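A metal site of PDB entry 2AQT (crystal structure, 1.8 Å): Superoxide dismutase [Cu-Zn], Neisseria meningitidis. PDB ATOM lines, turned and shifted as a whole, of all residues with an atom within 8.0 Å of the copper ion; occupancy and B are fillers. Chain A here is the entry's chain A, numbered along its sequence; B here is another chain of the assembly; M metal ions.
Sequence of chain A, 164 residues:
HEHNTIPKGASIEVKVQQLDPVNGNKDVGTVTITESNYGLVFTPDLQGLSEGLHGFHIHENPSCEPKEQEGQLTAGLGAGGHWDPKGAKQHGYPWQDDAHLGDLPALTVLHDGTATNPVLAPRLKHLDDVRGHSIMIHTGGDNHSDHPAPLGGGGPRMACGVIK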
ATOM      1  N   GLU A  51     -14.022 -10.547  21.832  1.00  0.00           N
ATOM      2  CA  GLU A  51     -14.435 -11.128  23.091  1.00  0.00           C
ATOM      3  C   GLU A  51     -15.755 -10.554  23.571  1.00  0.00           C
ATOM      4  O   GLU A  51     -16.070  -9.390  23.310  1.00  0.00           O
ATOM      5  CB  GLU A  51     -13.367 -10.909  24.172  1.00  0.00           C
ATOM      6  CG  GLU A  51     -13.381  -9.533  24.793  1.00  0.00           C
ATOM      7  CD  GLU A  51     -12.364  -9.377  25.909  1.00  0.00           C
ATOM      8  OE1 GLU A  51     -12.439 -10.130  26.915  1.00  0.00           O
ATOM      9  OE2 GLU A  51     -11.480  -8.508  25.781  1.00  0.00           O
ATOM     10  N   GLY A  52     -16.515 -11.375  24.295  1.00  0.00           N
ATOM     11  CA  GLY A  52     -17.794 -10.949  24.833  1.00  0.00           C
ATOM     12  C   GLY A  52     -18.946 -11.842  24.412  1.00  0.00           C
ATOM     13  O   GLY A  52     -18.762 -12.857  23.751  1.00  0.00           O
ATOM     14  N   VAL A 109     -17.599 -15.596  23.506  1.00  0.00           N
ATOM     15  CA  VAL A 109     -16.287 -15.552  22.860  1.00  0.00           C
ATOM     16  C   VAL A 109     -15.350 -15.094  23.969  1.00  0.00           C
ATOM     17  O   VAL A 109     -15.560 -14.042  24.573  1.00  0.00           O
ATOM     18  CB  VAL A 109     -16.238 -14.549  21.693  1.00  0.00           C
ATOM     19  CG1 VAL A 109     -14.824 -14.476  21.123  1.00  0.00           C
ATOM     20  CG2 VAL A 109     -17.219 -14.958  20.600  1.00  0.00           C
ATOM     21  N   LEU A 110     -14.322 -15.896  24.247  1.00  0.00           N
ATOM     22  CA  LEU A 110     -13.381 -15.571  25.319  1.00  0.00           C
ATOM     23  C   LEU A 110     -12.413 -14.452  24.952  1.00  0.00           C
ATOM     24  O   LEU A 110     -12.356 -14.017  23.815  1.00  0.00           O
ATOM     25  CB  LEU A 110     -12.591 -16.829  25.696  1.00  0.00           C
ATOM     26  CG  LEU A 110     -13.425 -17.993  26.248  1.00  0.00           C
ATOM     27  CD1 LEU A 110     -12.524 -19.202  26.435  1.00  0.00           C
ATOM     28  CD2 LEU A 110     -14.066 -17.579  27.573  1.00  0.00           C
ATOM     29  N   HIS A 111     -11.658 -14.003  25.951  1.00  0.00           N
ATOM     30  CA  HIS A 111     -10.672 -12.943  25.755  1.00  0.00           C
ATOM     31  C   HIS A 111      -9.741 -13.304  24.591  1.00  0.00           C
ATOM     32  O   HIS A 111      -9.343 -12.431  23.815  1.00  0.00           O
ATOM     33  CB  HIS A 111      -9.848 -12.749  27.029  1.00  0.00           C
ATOM     34  CG  HIS A 111      -8.870 -11.611  26.955  1.00  0.00           C
ATOM     35  ND1 HIS A 111      -9.219 -10.311  27.286  1.00  0.00           N
ATOM     36  CD2 HIS A 111      -7.587 -11.559  26.528  1.00  0.00           C
ATOM     37  CE1 HIS A 111      -8.181  -9.515  27.063  1.00  0.00           C
ATOM     38  NE2 HIS A 111      -7.180 -10.249  26.601  1.00  0.00           N
ATOM     39  N   ASP A 112      -9.407 -14.590  24.462  1.00  0.00           N
ATOM     40  CA  ASP A 112      -8.504 -15.037  23.408  1.00  0.00           C
ATOM     41  C   ASP A 112      -9.143 -15.164  22.019  1.00  0.00           C
ATOM     42  O   ASP A 112      -8.534 -15.696  21.089  1.00  0.00           O
ATOM     43  CB  ASP A 112      -7.837 -16.368  23.807  1.00  0.00           C
ATOM     44  CG  ASP A 112      -8.816 -17.532  23.843  1.00  0.00           C
ATOM     45  OD1 ASP A 112      -8.424 -18.603  24.338  1.00  0.00           O
ATOM     46  OD2 ASP A 112      -9.964 -17.386  23.374  1.00  0.00           O
ATOM     47  N   GLY A 113     -10.373 -14.677  21.891  1.00  0.00           N
ATOM     48  CA  GLY A 113     -11.063 -14.701  20.616  1.00  0.00           C
ATOM     49  C   GLY A 113     -11.686 -16.021  20.189  1.00  0.00           C
ATOM     50  O   GLY A 113     -12.173 -16.133  19.058  1.00  0.00           O
ATOM     51  N   GLU B  51     -12.556 -12.938  34.471  1.00  0.00           N
ATOM     52  CA  GLU B  51     -13.198 -13.167  33.178  1.00  0.00           C
ATOM     53  C   GLU B  51     -12.999 -14.595  32.680  1.00  0.00           C
ATOM     54  O   GLU B  51     -11.985 -15.237  32.961  1.00  0.00           O
ATOM     55  CB  GLU B  51     -12.666 -12.193  32.117  1.00  0.00           C
ATOM     56  CG  GLU B  51     -11.299 -12.549  31.547  1.00  0.00           C
ATOM     57  CD  GLU B  51     -10.857 -11.580  30.461  1.00  0.00           C
ATOM     58  OE1 GLU B  51     -11.631 -11.340  29.508  1.00  0.00           O
ATOM     59  OE2 GLU B  51      -9.727 -11.059  30.544  1.00  0.00           O
ATOM     60  N   GLY B  52     -13.996 -15.087  31.935  1.00  0.00           N
ATOM     61  CA  GLY B  52     -13.921 -16.428  31.395  1.00  0.00           C
ATOM     62  C   GLY B  52     -15.136 -17.273  31.720  1.00  0.00           C
ATOM     63  O   GLY B  52     -16.118 -16.780  32.278  1.00  0.00           O
ATOM     64  N   VAL B 109     -18.361 -14.902  32.582  1.00  0.00           N
ATOM     65  CA  VAL B 109     -17.965 -13.665  33.255  1.00  0.00           C
ATOM     66  C   VAL B 109     -17.209 -12.852  32.199  1.00  0.00           C
ATOM     67  O   VAL B 109     -16.222 -13.311  31.627  1.00  0.00           O
ATOM     68  CB  VAL B 109     -17.037 -13.932  34.467  1.00  0.00           C
ATOM     69  CG1 VAL B 109     -16.533 -12.609  35.052  1.00  0.00           C
ATOM     70  CG2 VAL B 109     -17.810 -14.689  35.549  1.00  0.00           C
ATOM     71  N   LEU B 110     -17.702 -11.644  31.940  1.00  0.00           N
ATOM     72  CA  LEU B 110     -17.122 -10.758  30.938  1.00  0.00           C
ATOM     73  C   LEU B 110     -15.822 -10.111  31.390  1.00  0.00           C
ATOM     74  O   LEU B 110     -15.414 -10.262  32.545  1.00  0.00           O
ATOM     75  CB  LEU B 110     -18.141  -9.680  30.568  1.00  0.00           C
ATOM     76  CG  LEU B 110     -19.440 -10.204  29.950  1.00  0.00           C
ATOM     77  CD1 LEU B 110     -20.433  -9.049  29.757  1.00  0.00           C
ATOM     78  CD2 LEU B 110     -19.144 -10.881  28.627  1.00  0.00           C
ATOM     79  N   HIS B 111     -15.185  -9.388  30.476  1.00  0.00           N
ATOM     80  CA  HIS B 111     -13.929  -8.717  30.767  1.00  0.00           C
ATOM     81  C   HIS B 111     -14.026  -7.827  32.000  1.00  0.00           C
ATOM     82  O   HIS B 111     -13.057  -7.676  32.751  1.00  0.00           O
ATOM     83  CB  HIS B 111     -13.491  -7.874  29.564  1.00  0.00           C
ATOM     84  CG  HIS B 111     -12.070  -7.438  29.627  1.00  0.00           C
ATOM     85  ND1 HIS B 111     -11.021  -8.282  29.316  1.00  0.00           N
ATOM     86  CD2 HIS B 111     -11.505  -6.265  30.005  1.00  0.00           C
ATOM     87  CE1 HIS B 111      -9.878  -7.642  29.502  1.00  0.00           C
ATOM     88  NE2 HIS B 111     -10.139  -6.415  29.921  1.00  0.00           N
ATOM     89  N   ASP B 112     -15.202  -7.227  32.205  1.00  0.00           N
ATOM     90  CA  ASP B 112     -15.387  -6.338  33.345  1.00  0.00           C
ATOM     91  C   ASP B 112     -15.721  -7.055  34.655  1.00  0.00           C
ATOM     92  O   ASP B 112     -16.076  -6.406  35.656  1.00  0.00           O
ATOM     93  CB  ASP B 112     -16.463  -5.288  33.038  1.00  0.00           C
ATOM     94  CG  ASP B 112     -17.838  -5.881  32.830  1.00  0.00           C
ATOM     95  OD1 ASP B 112     -18.778  -5.106  32.548  1.00  0.00           O
ATOM     96  OD2 ASP B 112     -17.977  -7.117  32.960  1.00  0.00           O
HETATM   97 CU    CU M   1     -10.958  -9.973  28.301  1.00  0.00          CU
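Within 4 Å of the copper ion: Glu 51 of chain A, His 111 of chain A, Glu 51 of chain B and His 111 of chain B. The nearest printed residue that does not touch the copper ion is Leu 110 of chain B (5.8 Å).
The copper ion is bound by the side-chain carboxylate (OE1) of Glu 51 of chain B, at 1.9 Å. The copper ion is bound by ND1 of His 111 of chain B, 2.0 Å away. OE1 of Glu 51 of chain A is bound to the copper ion, 2.0 Å away. ND1 of His 111 of chain A binds the copper ion. The copper ion has four donor atoms within binding distance. Slightly farther from the copper ion lies OE2 of Glu 51 of chain B (2.8 Å).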
